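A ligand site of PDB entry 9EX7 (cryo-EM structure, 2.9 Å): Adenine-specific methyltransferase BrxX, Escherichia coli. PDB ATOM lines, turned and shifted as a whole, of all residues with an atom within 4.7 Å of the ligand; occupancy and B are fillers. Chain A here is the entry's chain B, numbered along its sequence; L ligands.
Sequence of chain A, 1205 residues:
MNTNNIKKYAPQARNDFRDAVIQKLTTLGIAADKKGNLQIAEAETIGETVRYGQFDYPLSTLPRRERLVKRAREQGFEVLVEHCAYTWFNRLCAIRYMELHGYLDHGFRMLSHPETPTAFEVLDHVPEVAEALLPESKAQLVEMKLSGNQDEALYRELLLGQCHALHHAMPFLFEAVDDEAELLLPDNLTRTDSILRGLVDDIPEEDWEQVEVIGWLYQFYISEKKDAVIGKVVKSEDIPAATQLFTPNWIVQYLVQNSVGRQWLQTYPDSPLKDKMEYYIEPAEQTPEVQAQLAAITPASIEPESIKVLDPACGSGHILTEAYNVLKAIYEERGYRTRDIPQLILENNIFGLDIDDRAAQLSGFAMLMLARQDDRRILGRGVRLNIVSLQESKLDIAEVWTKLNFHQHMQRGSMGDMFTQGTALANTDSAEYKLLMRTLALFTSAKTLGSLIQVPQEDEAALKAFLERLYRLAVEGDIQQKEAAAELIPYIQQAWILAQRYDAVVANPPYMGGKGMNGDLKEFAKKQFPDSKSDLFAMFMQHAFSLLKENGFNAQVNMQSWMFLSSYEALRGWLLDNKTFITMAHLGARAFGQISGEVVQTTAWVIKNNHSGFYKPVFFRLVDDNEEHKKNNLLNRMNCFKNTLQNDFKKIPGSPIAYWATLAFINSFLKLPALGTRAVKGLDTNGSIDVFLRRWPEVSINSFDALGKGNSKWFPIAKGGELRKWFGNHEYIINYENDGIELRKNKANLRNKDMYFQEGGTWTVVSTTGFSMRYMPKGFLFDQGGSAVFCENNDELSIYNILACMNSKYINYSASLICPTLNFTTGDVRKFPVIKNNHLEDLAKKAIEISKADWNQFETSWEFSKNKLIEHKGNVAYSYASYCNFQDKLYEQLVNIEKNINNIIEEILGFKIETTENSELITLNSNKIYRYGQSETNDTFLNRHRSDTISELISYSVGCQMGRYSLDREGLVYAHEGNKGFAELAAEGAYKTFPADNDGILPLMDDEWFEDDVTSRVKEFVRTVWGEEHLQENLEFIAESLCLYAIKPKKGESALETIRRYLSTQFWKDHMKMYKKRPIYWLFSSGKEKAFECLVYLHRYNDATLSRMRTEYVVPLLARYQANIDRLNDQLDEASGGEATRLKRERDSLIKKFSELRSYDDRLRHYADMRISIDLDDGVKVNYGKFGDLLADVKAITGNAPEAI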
ATOM      1  N   TYR A 218      -9.376  15.181  31.414  1.00  0.00           N
ATOM      2  CA  TYR A 218     -10.463  14.523  30.693  1.00  0.00           C
ATOM      3  C   TYR A 218     -11.801  15.204  30.954  1.00  0.00           C
ATOM      4  O   TYR A 218     -12.628  15.336  30.047  1.00  0.00           O
ATOM      5  CB  TYR A 218     -10.513  13.046  31.101  1.00  0.00           C
ATOM      6  CG  TYR A 218     -11.737  12.283  30.654  1.00  0.00           C
ATOM      7  CD1 TYR A 218     -11.859  11.843  29.352  1.00  0.00           C
ATOM      8  CD2 TYR A 218     -12.758  11.987  31.541  1.00  0.00           C
ATOM      9  CE1 TYR A 218     -12.968  11.133  28.935  1.00  0.00           C
ATOM     10  CE2 TYR A 218     -13.868  11.288  31.143  1.00  0.00           C
ATOM     11  CZ  TYR A 218     -13.972  10.857  29.837  1.00  0.00           C
ATOM     12  OH  TYR A 218     -15.083  10.158  29.440  1.00  0.00           O
ATOM     13  N   ILE A 239     -23.241  12.812  21.785  1.00  0.00           N
ATOM     14  CA  ILE A 239     -23.448  11.881  22.899  1.00  0.00           C
ATOM     15  C   ILE A 239     -22.277  11.875  23.874  1.00  0.00           C
ATOM     16  O   ILE A 239     -22.505  11.998  25.086  1.00  0.00           O
ATOM     17  CB  ILE A 239     -23.780  10.479  22.369  1.00  0.00           C
ATOM     18  CG1 ILE A 239     -25.133  10.474  21.657  1.00  0.00           C
ATOM     19  CG2 ILE A 239     -23.772   9.472  23.490  1.00  0.00           C
ATOM     20  CD1 ILE A 239     -25.560   9.110  21.191  1.00  0.00           C
ATOM     21  N   PRO A 240     -21.015  11.724  23.437  1.00  0.00           N
ATOM     22  CA  PRO A 240     -19.924  11.752  24.419  1.00  0.00           C
ATOM     23  C   PRO A 240     -19.805  13.073  25.173  1.00  0.00           C
ATOM     24  O   PRO A 240     -19.456  13.068  26.359  1.00  0.00           O
ATOM     25  CB  PRO A 240     -18.680  11.477  23.568  1.00  0.00           C
ATOM     26  CG  PRO A 240     -19.064  11.894  22.193  1.00  0.00           C
ATOM     27  CD  PRO A 240     -20.506  11.513  22.071  1.00  0.00           C
ATOM     28  N   THR A 243     -22.278  13.193  28.472  1.00  0.00           N
ATOM     29  CA  THR A 243     -22.309  12.167  29.513  1.00  0.00           C
ATOM     30  C   THR A 243     -20.906  11.791  29.964  1.00  0.00           C
ATOM     31  O   THR A 243     -20.590  10.608  30.119  1.00  0.00           O
ATOM     32  CB  THR A 243     -23.049  10.915  29.019  1.00  0.00           C
ATOM     33  OG1 THR A 243     -22.450  10.449  27.810  1.00  0.00           O
ATOM     34  CG2 THR A 243     -24.519  11.223  28.770  1.00  0.00           C
ATOM     35  N   GLN A 244     -20.049  12.780  30.187  1.00  0.00           N
ATOM     36  CA  GLN A 244     -18.687  12.543  30.639  1.00  0.00           C
ATOM     37  C   GLN A 244     -18.493  13.189  32.007  1.00  0.00           C
ATOM     38  O   GLN A 244     -18.818  14.357  32.197  1.00  0.00           O
ATOM     39  CB  GLN A 244     -17.662  13.076  29.642  1.00  0.00           C
ATOM     40  CG  GLN A 244     -17.400  12.126  28.487  1.00  0.00           C
ATOM     41  CD  GLN A 244     -16.424  12.689  27.480  1.00  0.00           C
ATOM     42  OE1 GLN A 244     -15.949  13.817  27.608  1.00  0.00           O
ATOM     43  NE2 GLN A 244     -16.127  11.906  26.445  1.00  0.00           N
ATOM     44  N   LEU A 245     -17.944  12.415  32.947  1.00  0.00           N
ATOM     45  CA  LEU A 245     -17.832  12.832  34.327  1.00  0.00           C
ATOM     46  C   LEU A 245     -16.595  12.179  34.939  1.00  0.00           C
ATOM     47  O   LEU A 245     -15.826  11.499  34.251  1.00  0.00           O
ATOM     48  CB  LEU A 245     -19.104  12.479  35.094  1.00  0.00           C
ATOM     49  CG  LEU A 245     -19.521  13.399  36.239  1.00  0.00           C
ATOM     50  CD1 LEU A 245     -19.788  14.796  35.728  1.00  0.00           C
ATOM     51  CD2 LEU A 245     -20.748  12.849  36.944  1.00  0.00           C
ATOM     52  N   PHE A 246     -16.398  12.384  36.244  1.00  0.00           N
ATOM     53  CA  PHE A 246     -15.279  11.813  36.970  1.00  0.00           C
ATOM     54  C   PHE A 246     -15.804  11.179  38.255  1.00  0.00           C
ATOM     55  O   PHE A 246     -16.772  11.671  38.848  1.00  0.00           O
ATOM     56  CB  PHE A 246     -14.212  12.867  37.286  1.00  0.00           C
ATOM     57  CG  PHE A 246     -12.933  12.309  37.823  1.00  0.00           C
ATOM     58  CD1 PHE A 246     -12.110  11.539  37.019  1.00  0.00           C
ATOM     59  CD2 PHE A 246     -12.540  12.569  39.121  1.00  0.00           C
ATOM     60  CE1 PHE A 246     -10.927  11.030  37.516  1.00  0.00           C
ATOM     61  CE2 PHE A 246     -11.366  12.056  39.620  1.00  0.00           C
ATOM     62  CZ  PHE A 246     -10.552  11.283  38.818  1.00  0.00           C
ATOM     63  N   THR A 247     -15.161  10.095  38.682  1.00  0.00           N
ATOM     64  CA  THR A 247     -15.651   9.322  39.805  1.00  0.00           C
ATOM     65  C   THR A 247     -14.691   9.393  40.984  1.00  0.00           C
ATOM     66  O   THR A 247     -13.479   9.204  40.785  1.00  0.00           O
ATOM     67  CB  THR A 247     -15.865   7.857  39.396  1.00  0.00           C
ATOM     68  OG1 THR A 247     -16.628   7.806  38.190  1.00  0.00           O
ATOM     69  CG2 THR A 247     -16.605   7.105  40.484  1.00  0.00           C
ATOM     70  N   PRO A 312     -17.292  -1.726  30.337  1.00  0.00           N
ATOM     71  CA  PRO A 312     -18.019  -1.319  29.137  1.00  0.00           C
ATOM     72  C   PRO A 312     -17.900   0.155  28.796  1.00  0.00           C
ATOM     73  O   PRO A 312     -18.168   0.525  27.639  1.00  0.00           O
ATOM     74  CB  PRO A 312     -19.471  -1.698  29.458  1.00  0.00           C
ATOM     75  CG  PRO A 312     -19.366  -2.726  30.511  1.00  0.00           C
ATOM     76  CD  PRO A 312     -18.187  -2.347  31.336  1.00  0.00           C
ATOM     77  N   ALA A 313     -17.541   1.008  29.749  1.00  0.00           N
ATOM     78  CA  ALA A 313     -17.356   2.442  29.492  1.00  0.00           C
ATOM     79  C   ALA A 313     -16.058   2.858  30.199  1.00  0.00           C
ATOM     80  O   ALA A 313     -16.070   3.180  31.392  1.00  0.00           O
ATOM     81  CB  ALA A 313     -18.553   3.251  29.990  1.00  0.00           C
ATOM     82  N   CYS A 314     -14.962   2.847  29.446  1.00  0.00           N
ATOM     83  CA  CYS A 314     -13.651   3.112  30.032  1.00  0.00           C
ATOM     84  C   CYS A 314     -13.565   4.526  30.593  1.00  0.00           C
ATOM     85  O   CYS A 314     -13.204   4.728  31.747  1.00  0.00           O
ATOM     86  CB  CYS A 314     -12.547   2.881  29.008  1.00  0.00           C
ATOM     87  SG  CYS A 314     -12.376   1.181  28.460  1.00  0.00           S
ATOM     88  N   GLY A 315     -13.900   5.514  29.771  1.00  0.00           N
ATOM     89  CA  GLY A 315     -13.722   6.892  30.195  1.00  0.00           C
ATOM     90  C   GLY A 315     -12.255   7.208  30.416  1.00  0.00           C
ATOM     91  O   GLY A 315     -11.407   6.967  29.552  1.00  0.00           O
ATOM     92  N   SER A 316     -11.939   7.737  31.596  1.00  0.00           N
ATOM     93  CA  SER A 316     -10.565   8.096  31.909  1.00  0.00           C
ATOM     94  C   SER A 316      -9.712   6.869  32.206  1.00  0.00           C
ATOM     95  O   SER A 316      -8.486   6.920  32.018  1.00  0.00           O
ATOM     96  CB  SER A 316     -10.525   9.056  33.097  1.00  0.00           C
ATOM     97  OG  SER A 316      -9.202   9.260  33.528  1.00  0.00           O
ATOM     98  N   HIS A 318     -10.204   4.977  35.412  1.00  0.00           N
ATOM     99  CA  HIS A 318      -9.970   4.962  36.857  1.00  0.00           C
ATOM    100  C   HIS A 318     -10.134   3.566  37.452  1.00  0.00           C
ATOM    101  O   HIS A 318      -9.389   3.206  38.373  1.00  0.00           O
ATOM    102  CB  HIS A 318     -10.916   5.951  37.535  1.00  0.00           C
ATOM    103  CG  HIS A 318     -10.467   6.400  38.882  1.00  0.00           C
ATOM    104  ND1 HIS A 318     -11.175   7.290  39.643  1.00  0.00           N
ATOM    105  CD2 HIS A 318      -9.375   6.079  39.606  1.00  0.00           C
ATOM    106  CE1 HIS A 318     -10.544   7.504  40.780  1.00  0.00           C
ATOM    107  NE2 HIS A 318      -9.439   6.779  40.787  1.00  0.00           N
ATOM    108  N   ASP A 354     -15.127   1.707  24.692  1.00  0.00           N
ATOM    109  CA  ASP A 354     -15.697   3.036  24.801  1.00  0.00           C
ATOM    110  C   ASP A 354     -16.216   3.461  23.442  1.00  0.00           C
ATOM    111  O   ASP A 354     -16.034   2.770  22.439  1.00  0.00           O
ATOM    112  CB  ASP A 354     -14.668   4.040  25.341  1.00  0.00           C
ATOM    113  CG  ASP A 354     -15.319   5.260  25.960  1.00  0.00           C
ATOM    114  OD1 ASP A 354     -16.342   5.721  25.424  1.00  0.00           O
ATOM    115  OD2 ASP A 354     -14.801   5.749  26.988  1.00  0.00           O
ATOM    116  N   ILE A 355     -16.878   4.624  23.420  1.00  0.00           N
ATOM    117  CA  ILE A 355     -17.483   5.142  22.193  1.00  0.00           C
ATOM    118  C   ILE A 355     -16.694   6.294  21.594  1.00  0.00           C
ATOM    119  O   ILE A 355     -16.952   6.668  20.436  1.00  0.00           O
ATOM    120  CB  ILE A 355     -18.937   5.591  22.456  1.00  0.00           C
ATOM    121  CG1 ILE A 355     -19.764   5.502  21.169  1.00  0.00           C
ATOM    122  CG2 ILE A 355     -18.972   6.999  23.006  1.00  0.00           C
ATOM    123  CD1 ILE A 355     -19.875   4.103  20.628  1.00  0.00           C
ATOM    124  N   ASP A 356     -15.728   6.851  22.310  1.00  0.00           N
ATOM    125  CA  ASP A 356     -14.957   8.004  21.858  1.00  0.00           C
ATOM    126  C   ASP A 356     -13.480   7.661  21.809  1.00  0.00           C
ATOM    127  O   ASP A 356     -12.981   6.859  22.592  1.00  0.00           O
ATOM    128  CB  ASP A 356     -15.189   9.206  22.774  1.00  0.00           C
ATOM    129  CG  ASP A 356     -14.708  10.513  22.158  1.00  0.00           C
ATOM    130  OD1 ASP A 356     -13.687  10.513  21.446  1.00  0.00           O
ATOM    131  OD2 ASP A 356     -15.366  11.550  22.396  1.00  0.00           O
ATOM    132  N   THR A 448     -23.916   5.090  17.442  1.00  0.00           N
ATOM    133  CA  THR A 448     -25.116   5.460  18.167  1.00  0.00           C
ATOM    134  C   THR A 448     -25.489   4.467  19.257  1.00  0.00           C
ATOM    135  O   THR A 448     -25.805   4.888  20.373  1.00  0.00           O
ATOM    136  CB  THR A 448     -26.299   5.588  17.195  1.00  0.00           C
ATOM    137  OG1 THR A 448     -25.965   6.516  16.158  1.00  0.00           O
ATOM    138  CG2 THR A 448     -27.537   6.068  17.928  1.00  0.00           C
ATOM    139  N   LEU A 449     -25.432   3.166  18.972  1.00  0.00           N
ATOM    140  CA  LEU A 449     -25.805   2.163  19.970  1.00  0.00           C
ATOM    141  C   LEU A 449     -24.700   1.983  20.997  1.00  0.00           C
ATOM    142  O   LEU A 449     -24.905   2.195  22.201  1.00  0.00           O
ATOM    143  CB  LEU A 449     -26.125   0.843  19.283  1.00  0.00           C
ATOM    144  CG  LEU A 449     -27.243   0.902  18.241  1.00  0.00           C
ATOM    145  CD1 LEU A 449     -27.511  -0.481  17.680  1.00  0.00           C
ATOM    146  CD2 LEU A 449     -28.488   1.491  18.842  1.00  0.00           C
ATOM    147  N   GLY A 450     -23.509   1.595  20.552  1.00  0.00           N
ATOM    148  CA  GLY A 450     -22.375   1.445  21.446  1.00  0.00           C
ATOM    149  C   GLY A 450     -22.171  -0.001  21.856  1.00  0.00           C
ATOM    150  O   GLY A 450     -22.164  -0.899  21.022  1.00  0.00           O
ATOM    151  N   SER A 451     -22.021  -0.226  23.165  1.00  0.00           N
ATOM    152  CA  SER A 451     -21.730  -1.543  23.700  1.00  0.00           C
ATOM    153  C   SER A 451     -22.977  -2.397  23.884  1.00  0.00           C
ATOM    154  O   SER A 451     -22.876  -3.479  24.470  1.00  0.00           O
ATOM    155  CB  SER A 451     -20.990  -1.416  25.036  1.00  0.00           C
ATOM    156  OG  SER A 451     -19.804  -0.659  24.885  1.00  0.00           O
ATOM    157  N   ASN A 508     -19.669   2.604  35.202  1.00  0.00           N
ATOM    158  CA  ASN A 508     -20.436   3.780  35.622  1.00  0.00           C
ATOM    159  C   ASN A 508     -21.268   4.199  34.426  1.00  0.00           C
ATOM    160  O   ASN A 508     -20.808   4.976  33.580  1.00  0.00           O
ATOM    161  CB  ASN A 508     -19.525   4.900  36.110  1.00  0.00           C
ATOM    162  CG  ASN A 508     -20.283   6.057  36.714  1.00  0.00           C
ATOM    163  OD1 ASN A 508     -21.467   6.249  36.454  1.00  0.00           O
ATOM    164  ND2 ASN A 508     -19.605   6.843  37.534  1.00  0.00           N
ATOM    165  N   PRO A 510     -23.672   5.859  31.646  1.00  0.00           N
ATOM    166  CA  PRO A 510     -24.107   7.234  31.385  1.00  0.00           C
ATOM    167  C   PRO A 510     -25.590   7.416  31.666  1.00  0.00           C
ATOM    168  O   PRO A 510     -26.386   6.476  31.594  1.00  0.00           O
ATOM    169  CB  PRO A 510     -23.802   7.419  29.897  1.00  0.00           C
ATOM    170  CG  PRO A 510     -23.888   6.054  29.340  1.00  0.00           C
ATOM    171  CD  PRO A 510     -23.352   5.136  30.399  1.00  0.00           C
ATOM    172  N   PHE A 540     -28.127  -0.664  30.374  1.00  0.00           N
ATOM    173  CA  PHE A 540     -26.756  -1.092  30.635  1.00  0.00           C
ATOM    174  C   PHE A 540     -26.718  -2.192  31.688  1.00  0.00           C
ATOM    175  O   PHE A 540     -25.943  -3.152  31.554  1.00  0.00           O
ATOM    176  CB  PHE A 540     -25.909   0.102  31.083  1.00  0.00           C
ATOM    177  CG  PHE A 540     -24.995   0.608  30.021  1.00  0.00           C
ATOM    178  CD1 PHE A 540     -23.730   0.076  29.856  1.00  0.00           C
ATOM    179  CD2 PHE A 540     -25.390   1.616  29.163  1.00  0.00           C
ATOM    180  CE1 PHE A 540     -22.883   0.540  28.874  1.00  0.00           C
ATOM    181  CE2 PHE A 540     -24.558   2.088  28.180  1.00  0.00           C
ATOM    182  CZ  PHE A 540     -23.298   1.550  28.039  1.00  0.00           C
HETATM  183  N1  LIG L   1     -16.276   5.237  34.014  1.00  0.00           N
HETATM  184  C1  LIG L   1     -15.449   6.408  33.734  1.00  0.00           C
HETATM  185  C2  LIG L   1     -15.007   7.091  35.023  1.00  0.00           C
HETATM  186  O1  LIG L   1     -13.986   7.767  35.048  1.00  0.00           O
HETATM  187  O2  LIG L   1     -15.664   6.985  36.057  1.00  0.00           O
HETATM  188  C3  LIG L   1     -16.195   7.389  32.845  1.00  0.00           C
HETATM  189  C4  LIG L   1     -17.703   7.426  33.050  1.00  0.00           C
HETATM  190  S1  LIG L   1     -18.502   8.604  31.940  1.00  0.00           S
HETATM  191  C5  LIG L   1     -19.819   9.219  33.013  1.00  0.00           C
HETATM  192  C6  LIG L   1     -19.439   7.498  30.849  1.00  0.00           C
HETATM  193  C7  LIG L   1     -18.684   7.154  29.579  1.00  0.00           C
HETATM  194  O3  LIG L   1     -19.410   6.204  28.821  1.00  0.00           O
HETATM  195  C8  LIG L   1     -18.477   8.363  28.680  1.00  0.00           C
HETATM  196  O4  LIG L   1     -17.112   8.715  28.669  1.00  0.00           O
HETATM  197  C9  LIG L   1     -18.884   7.905  27.295  1.00  0.00           C
HETATM  198  O5  LIG L   1     -17.794   8.052  26.414  1.00  0.00           O
HETATM  199  C10 LIG L   1     -19.229   6.435  27.442  1.00  0.00           C
HETATM  200  N2  LIG L   1     -20.459   6.103  26.705  1.00  0.00           N
HETATM  201  C11 LIG L   1     -21.547   6.915  26.518  1.00  0.00           C
HETATM  202  N3  LIG L   1     -22.463   6.243  25.787  1.00  0.00           N
HETATM  203  C12 LIG L   1     -21.973   5.020  25.501  1.00  0.00           C
HETATM  204  C13 LIG L   1     -22.499   3.945  24.792  1.00  0.00           C
HETATM  205  N4  LIG L   1     -23.711   4.040  24.250  1.00  0.00           N
HETATM  206  N5  LIG L   1     -21.762   2.798  24.651  1.00  0.00           N
HETATM  207  C14 LIG L   1     -20.516   2.717  25.224  1.00  0.00           C
HETATM  208  N6  LIG L   1     -19.997   3.779  25.930  1.00  0.00           N
HETATM  209  C15 LIG L   1     -20.717   4.910  26.065  1.00  0.00           C
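O of Thr 243 sits close to S1 of the ligand (3.4 Å). Merely in contact with the ligand: Gln 244 (3.4 Å), Leu 245 (3.7 Å), Cys 314 (3.4 Å), Gly 315 (3.7 Å), Ile 355 (3.8 Å), Gly 450 (3.5 Å), Asn 508 (3.9 Å), Pro 510 (3.8 Å) and Phe 540 (3.9 Å). Within 4 Å of the ligand: Tyr 218, Thr 243, Gln 244, Leu 245, Thr 247, Ala 313, Cys 314, Gly 315, Asp 354, Ile 355, Leu 449, Gly 450, Ser 451, Asn 508, Pro 510 and Phe 540. Along chain A the residues within 4 Å of the ligand span positions 218 to 540.
The backbone carbonyl oxygen (O) of Ala 313 is in hydrogen-bond range of a nitrogen (N1) of the ligand, at 3.3 Å. The side-chain carboxylate (OD1) of Asp 354 sits at hydrogen-bond distance from an oxygen (O5) of the ligand, 2.9 Å away. O2 of the ligand sits at hydrogen-bond distance from OG1 of Thr 247. OH of Tyr 218 is in hydrogen-bond range of O4 of the ligand (2.6 Å). N5 of the ligand lies within hydrogen-bond range of N of Ser 451 (3.4 Å). The backbone carbonyl oxygen (O) of Leu 449 sits at hydrogen-bond distance from a nitrogen (N4) of the ligand (3.0 Å).
The backbone carbonyl oxygen of Ile 239 is in hydrogen-bond range of the side-chain hydroxyl of Thr 243 (3.1 Å). The backbone NH of Gly 315 lies within hydrogen-bond range of the side-chain carboxylate of Asp 354 (2.9 Å). OG of Ser 451 is in hydrogen-bond range of O of Pro 312. The backbone NH (N) of Asp 356 is in hydrogen-bond range of the side-chain carboxylate (OD1) of Asp 354 (3.4 Å). The side-chain amide nitrogen (ND2) of Asn 508 sits at hydrogen-bond distance from the side-chain hydroxyl (OG1) of Thr 247, at 3.2 Å. The backbone carbonyl oxygen (O) of Thr 247 is in hydrogen-bond range of a ring nitrogen (ND1) of His 318.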
